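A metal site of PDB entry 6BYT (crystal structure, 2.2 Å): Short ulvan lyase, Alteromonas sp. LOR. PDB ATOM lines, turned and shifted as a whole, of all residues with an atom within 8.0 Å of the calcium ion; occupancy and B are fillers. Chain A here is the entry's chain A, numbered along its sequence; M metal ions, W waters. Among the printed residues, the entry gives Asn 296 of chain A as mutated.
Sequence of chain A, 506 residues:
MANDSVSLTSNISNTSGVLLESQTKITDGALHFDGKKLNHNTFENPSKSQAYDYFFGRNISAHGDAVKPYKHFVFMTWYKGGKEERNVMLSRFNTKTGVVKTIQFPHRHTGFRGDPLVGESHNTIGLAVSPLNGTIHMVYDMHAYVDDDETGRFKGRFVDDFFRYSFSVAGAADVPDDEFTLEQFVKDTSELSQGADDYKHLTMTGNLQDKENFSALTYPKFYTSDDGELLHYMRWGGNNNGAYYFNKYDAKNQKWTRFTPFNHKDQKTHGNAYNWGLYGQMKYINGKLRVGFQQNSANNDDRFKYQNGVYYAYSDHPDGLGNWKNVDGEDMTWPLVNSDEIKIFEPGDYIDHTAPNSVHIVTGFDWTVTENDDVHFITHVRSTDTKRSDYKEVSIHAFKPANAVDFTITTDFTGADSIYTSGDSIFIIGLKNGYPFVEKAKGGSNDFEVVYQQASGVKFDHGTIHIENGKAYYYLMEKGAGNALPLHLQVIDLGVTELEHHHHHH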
ATOM      1  N   ASN A 240     -16.172  -4.926   9.368  1.00  0.00           N
ATOM      2  CA  ASN A 240     -15.832  -5.504  10.659  1.00  0.00           C
ATOM      3  C   ASN A 240     -14.970  -6.748  10.485  1.00  0.00           C
ATOM      4  O   ASN A 240     -14.940  -7.651  11.343  1.00  0.00           O
ATOM      5  CB  ASN A 240     -17.102  -5.799  11.450  1.00  0.00           C
ATOM      6  CG  ASN A 240     -18.116  -6.557  10.660  1.00  0.00           C
ATOM      7  OD1 ASN A 240     -17.791  -7.554  10.010  1.00  0.00           O
ATOM      8  ND2 ASN A 240     -19.373  -6.106  10.713  1.00  0.00           N
ATOM      9  N   GLN A 295     -10.933   0.653  15.747  1.00  0.00           N
ATOM     10  CA  GLN A 295     -11.394  -0.648  15.290  1.00  0.00           C
ATOM     11  C   GLN A 295     -12.903  -0.648  15.117  1.00  0.00           C
ATOM     12  O   GLN A 295     -13.629   0.137  15.731  1.00  0.00           O
ATOM     13  CB  GLN A 295     -10.985  -1.747  16.264  1.00  0.00           C
ATOM     14  CG  GLN A 295     -11.908  -1.826  17.464  1.00  0.00           C
ATOM     15  CD  GLN A 295     -11.777  -3.113  18.279  1.00  0.00           C
ATOM     16  OE1 GLN A 295     -10.874  -3.919  18.051  1.00  0.00           O
ATOM     17  NE2 GLN A 295     -12.697  -3.322  19.208  1.00  0.00           N
ATOM     18  N   ASN A 296     -13.383  -1.576  14.283  1.00  0.00           N
ATOM     19  CA  ASN A 296     -14.820  -1.797  14.112  1.00  0.00           C
ATOM     20  C   ASN A 296     -15.060  -3.284  14.399  1.00  0.00           C
ATOM     21  O   ASN A 296     -14.967  -4.136  13.506  1.00  0.00           O
ATOM     22  CB  ASN A 296     -15.283  -1.419  12.745  1.00  0.00           C
ATOM     23  CG  ASN A 296     -16.806  -1.335  12.645  1.00  0.00           C
ATOM     24  OD1 ASN A 296     -17.491  -2.355  12.720  1.00  0.00           O
ATOM     25  ND2 ASN A 296     -17.324  -0.134  12.459  1.00  0.00           N
ATOM     26  N   SER A 297     -15.334  -3.600  15.665  1.00  0.00           N
ATOM     27  CA  SER A 297     -15.537  -4.996  16.009  1.00  0.00           C
ATOM     28  C   SER A 297     -16.781  -5.534  15.331  1.00  0.00           C
ATOM     29  O   SER A 297     -17.736  -4.794  15.042  1.00  0.00           O
ATOM     30  CB  SER A 297     -15.672  -5.170  17.530  1.00  0.00           C
ATOM     31  OG  SER A 297     -16.137  -6.478  17.824  1.00  0.00           O
ATOM     32  N   ALA A 298     -16.757  -6.842  15.027  1.00  0.00           N
ATOM     33  CA  ALA A 298     -17.932  -7.551  14.526  1.00  0.00           C
ATOM     34  C   ALA A 298     -18.981  -7.779  15.607  1.00  0.00           C
ATOM     35  O   ALA A 298     -20.106  -8.174  15.285  1.00  0.00           O
ATOM     36  CB  ALA A 298     -17.546  -8.918  13.949  1.00  0.00           C
ATOM     37  N   ASN A 299     -18.641  -7.554  16.867  1.00  0.00           N
ATOM     38  CA  ASN A 299     -19.627  -7.669  17.933  1.00  0.00           C
ATOM     39  C   ASN A 299     -20.706  -6.591  17.755  1.00  0.00           C
ATOM     40  O   ASN A 299     -20.395  -5.394  17.660  1.00  0.00           O
ATOM     41  CB  ASN A 299     -18.947  -7.504  19.297  1.00  0.00           C
ATOM     42  CG  ASN A 299     -19.890  -7.680  20.453  1.00  0.00           C
ATOM     43  OD1 ASN A 299     -21.059  -7.957  20.265  1.00  0.00           O
ATOM     44  ND2 ASN A 299     -19.379  -7.515  21.673  1.00  0.00           N
ATOM     45  N   ASN A 300     -21.966  -7.017  17.699  1.00  0.00           N
ATOM     46  CA  ASN A 300     -23.097  -6.118  17.572  1.00  0.00           C
ATOM     47  C   ASN A 300     -23.941  -6.057  18.835  1.00  0.00           C
ATOM     48  O   ASN A 300     -25.068  -5.578  18.795  1.00  0.00           O
ATOM     49  CB  ASN A 300     -23.985  -6.507  16.383  1.00  0.00           C
ATOM     50  CG  ASN A 300     -23.259  -6.400  15.071  1.00  0.00           C
ATOM     51  OD1 ASN A 300     -22.360  -5.567  14.917  1.00  0.00           O
ATOM     52  ND2 ASN A 300     -23.636  -7.230  14.096  1.00  0.00           N
ATOM     53  N   ASP A 301     -23.409  -6.546  19.967  1.00  0.00           N
ATOM     54  CA  ASP A 301     -24.130  -6.508  21.228  1.00  0.00           C
ATOM     55  C   ASP A 301     -23.567  -5.515  22.224  1.00  0.00           C
ATOM     56  O   ASP A 301     -24.240  -5.227  23.224  1.00  0.00           O
ATOM     57  CB  ASP A 301     -24.141  -7.898  21.883  1.00  0.00           C
ATOM     58  CG  ASP A 301     -25.033  -8.892  21.146  1.00  0.00           C
ATOM     59  OD1 ASP A 301     -25.997  -8.472  20.470  1.00  0.00           O
ATOM     60  OD2 ASP A 301     -24.758 -10.106  21.254  1.00  0.00           O
ATOM     61  N   ASP A 302     -22.374  -4.969  21.989  1.00  0.00           N
ATOM     62  CA  ASP A 302     -21.783  -4.002  22.900  1.00  0.00           C
ATOM     63  C   ASP A 302     -22.299  -2.602  22.571  1.00  0.00           C
ATOM     64  O   ASP A 302     -23.196  -2.447  21.731  1.00  0.00           O
ATOM     65  CB  ASP A 302     -20.260  -4.073  22.864  1.00  0.00           C
ATOM     66  CG  ASP A 302     -19.669  -3.609  21.535  1.00  0.00           C
ATOM     67  OD1 ASP A 302     -20.412  -3.239  20.597  1.00  0.00           O
ATOM     68  OD2 ASP A 302     -18.413  -3.614  21.431  1.00  0.00           O
ATOM     69  N   ARG A 303     -21.737  -1.572  23.219  1.00  0.00           N
ATOM     70  CA  ARG A 303     -22.324  -0.233  23.160  1.00  0.00           C
ATOM     71  C   ARG A 303     -21.959   0.543  21.904  1.00  0.00           C
ATOM     72  O   ARG A 303     -22.547   1.600  21.656  1.00  0.00           O
ATOM     73  CB  ARG A 303     -21.903   0.615  24.384  1.00  0.00           C
ATOM     74  CG  ARG A 303     -20.467   1.129  24.299  1.00  0.00           C
ATOM     75  CD  ARG A 303     -19.958   1.750  25.600  1.00  0.00           C
ATOM     76  NE  ARG A 303     -19.843   0.800  26.693  1.00  0.00           N
ATOM     77  CZ  ARG A 303     -19.647   1.158  27.960  1.00  0.00           C
ATOM     78  NH1 ARG A 303     -19.577   2.438  28.291  1.00  0.00           N
ATOM     79  NH2 ARG A 303     -19.563   0.223  28.913  1.00  0.00           N
ATOM     80  N   PHE A 304     -20.981   0.061  21.114  1.00  0.00           N
ATOM     81  CA  PHE A 304     -20.442   0.808  19.967  1.00  0.00           C
ATOM     82  C   PHE A 304     -21.114   0.309  18.693  1.00  0.00           C
ATOM     83  O   PHE A 304     -20.872  -0.827  18.267  1.00  0.00           O
ATOM     84  CB  PHE A 304     -18.922   0.654  19.885  1.00  0.00           C
ATOM     85  CG  PHE A 304     -18.218   1.037  21.147  1.00  0.00           C
ATOM     86  CD1 PHE A 304     -17.986   2.372  21.445  1.00  0.00           C
ATOM     87  CD2 PHE A 304     -17.815   0.073  22.052  1.00  0.00           C
ATOM     88  CE1 PHE A 304     -17.343   2.725  22.623  1.00  0.00           C
ATOM     89  CE2 PHE A 304     -17.194   0.425  23.227  1.00  0.00           C
ATOM     90  CZ  PHE A 304     -16.951   1.753  23.508  1.00  0.00           C
ATOM     91  N   LYS A 305     -21.928   1.168  18.068  1.00  0.00           N
ATOM     92  CA  LYS A 305     -22.579   0.764  16.828  1.00  0.00           C
ATOM     93  C   LYS A 305     -21.562   0.483  15.724  1.00  0.00           C
ATOM     94  O   LYS A 305     -21.685  -0.512  14.998  1.00  0.00           O
ATOM     95  CB  LYS A 305     -23.574   1.831  16.384  1.00  0.00           C
ATOM     96  CG  LYS A 305     -24.577   1.317  15.340  1.00  0.00           C
ATOM     97  CD  LYS A 305     -25.541   2.397  14.929  1.00  0.00           C
ATOM     98  CE  LYS A 305     -26.632   1.862  14.002  1.00  0.00           C
ATOM     99  NZ  LYS A 305     -27.634   2.920  13.622  1.00  0.00           N
ATOM    100  N   TYR A 306     -20.530   1.328  15.593  1.00  0.00           N
ATOM    101  CA  TYR A 306     -19.506   1.134  14.575  1.00  0.00           C
ATOM    102  C   TYR A 306     -18.159   1.052  15.260  1.00  0.00           C
ATOM    103  O   TYR A 306     -17.797  -0.004  15.798  1.00  0.00           O
ATOM    104  CB  TYR A 306     -19.617   2.241  13.512  1.00  0.00           C
ATOM    105  CG  TYR A 306     -20.957   2.251  12.812  1.00  0.00           C
ATOM    106  CD1 TYR A 306     -21.344   1.203  11.973  1.00  0.00           C
ATOM    107  CD2 TYR A 306     -21.840   3.317  12.990  1.00  0.00           C
ATOM    108  CE1 TYR A 306     -22.581   1.217  11.316  1.00  0.00           C
ATOM    109  CE2 TYR A 306     -23.091   3.328  12.342  1.00  0.00           C
ATOM    110  CZ  TYR A 306     -23.433   2.283  11.508  1.00  0.00           C
ATOM    111  OH  TYR A 306     -24.655   2.296  10.883  1.00  0.00           O
ATOM    112  N   GLN A 307     -17.362   2.109  15.252  1.00  0.00           N
ATOM    113  CA  GLN A 307     -15.988   2.038  15.722  1.00  0.00           C
ATOM    114  C   GLN A 307     -15.872   2.267  17.221  1.00  0.00           C
ATOM    115  O   GLN A 307     -16.780   2.776  17.890  1.00  0.00           O
ATOM    116  CB  GLN A 307     -15.111   3.060  14.991  1.00  0.00           C
ATOM    117  CG  GLN A 307     -14.933   2.703  13.523  1.00  0.00           C
ATOM    118  CD  GLN A 307     -14.712   3.913  12.664  1.00  0.00           C
ATOM    119  OE1 GLN A 307     -13.979   4.846  13.034  1.00  0.00           O
ATOM    120  NE2 GLN A 307     -15.376   3.952  11.527  1.00  0.00           N
ATOM    121  N   ASN A 308     -14.715   1.872  17.761  1.00  0.00           N
ATOM    122  CA  ASN A 308     -14.402   2.173  19.146  1.00  0.00           C
ATOM    123  C   ASN A 308     -12.894   2.236  19.295  1.00  0.00           C
ATOM    124  O   ASN A 308     -12.153   1.742  18.449  1.00  0.00           O
ATOM    125  CB  ASN A 308     -14.993   1.134  20.110  1.00  0.00           C
ATOM    126  CG  ASN A 308     -14.188  -0.160  20.165  1.00  0.00           C
ATOM    127  OD1 ASN A 308     -14.354  -1.054  19.321  1.00  0.00           O
ATOM    128  ND2 ASN A 308     -13.303  -0.264  21.168  1.00  0.00           N
ATOM    129  N   PRO A 356     -26.602  -1.289  24.307  1.00  0.00           N
ATOM    130  CA  PRO A 356     -26.050  -1.783  23.047  1.00  0.00           C
ATOM    131  C   PRO A 356     -26.249  -0.793  21.904  1.00  0.00           C
ATOM    132  O   PRO A 356     -27.347  -0.273  21.705  1.00  0.00           O
ATOM    133  CB  PRO A 356     -26.815  -3.089  22.821  1.00  0.00           C
ATOM    134  CG  PRO A 356     -27.249  -3.534  24.227  1.00  0.00           C
ATOM    135  CD  PRO A 356     -27.547  -2.230  24.941  1.00  0.00           C
ATOM    136  N   ASN A 357     -25.172  -0.536  21.170  1.00  0.00           N
ATOM    137  CA  ASN A 357     -25.187   0.271  19.943  1.00  0.00           C
ATOM    138  C   ASN A 357     -25.563   1.724  20.164  1.00  0.00           C
ATOM    139  O   ASN A 357     -25.826   2.439  19.204  1.00  0.00           O
ATOM    140  CB  ASN A 357     -26.140  -0.330  18.912  1.00  0.00           C
ATOM    141  CG  ASN A 357     -25.771  -1.734  18.557  1.00  0.00           C
ATOM    142  OD1 ASN A 357     -24.690  -1.967  18.037  1.00  0.00           O
ATOM    143  ND2 ASN A 357     -26.648  -2.677  18.860  1.00  0.00           N
ATOM    144  N   VAL A 359     -23.592   4.157  21.107  1.00  0.00           N
ATOM    145  CA  VAL A 359     -22.452   5.057  20.937  1.00  0.00           C
ATOM    146  C   VAL A 359     -21.998   4.999  19.482  1.00  0.00           C
ATOM    147  O   VAL A 359     -21.707   3.904  18.961  1.00  0.00           O
ATOM    148  CB  VAL A 359     -21.295   4.701  21.880  1.00  0.00           C
ATOM    149  CG1 VAL A 359     -20.080   5.577  21.622  1.00  0.00           C
ATOM    150  CG2 VAL A 359     -21.738   4.809  23.326  1.00  0.00           C
HETATM  151 CA    CA M   1     -20.482  -3.107  18.114  1.00  0.00          CA
HETATM  152  O   HOH W   1     -18.025  -3.096  18.904  1.00  0.00           O
HETATM  153  O   HOH W   2     -22.826  -3.391  18.998  1.00  0.00           O
HETATM  154  O   HOH W   3     -19.178  -2.601  15.887  1.00  0.00           O
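N of Asn 299 sits at hydrogen-bond distance from OG of Ser 297, at 2.9 Å.
OD1 of Asn 299 sits at hydrogen-bond distance from N of Asp 301 (2.8 Å).
O of Asp 302 lies within hydrogen-bond range of N of Asn 357 (2.8 Å).
Of the 18 residues printed, 3 come within 4 Å of the calcium ion.
The nearest printed residue that does not touch the calcium ion is Asn 300 (4.02 Å).
O of Phe 304 binds the calcium ion, 2.3 Å away.
O of Asn 299 is bound to the calcium ion, 2.3 Å away.
The calcium ion is bound by the side-chain carboxylate (OD1) of Asp 302 (2.5 Å).
Water W2 binds the calcium ion (2.5 Å).
Water W1 binds the calcium ion (2.6 Å).
The calcium ion is bound by water W3, 2.6 Å away.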
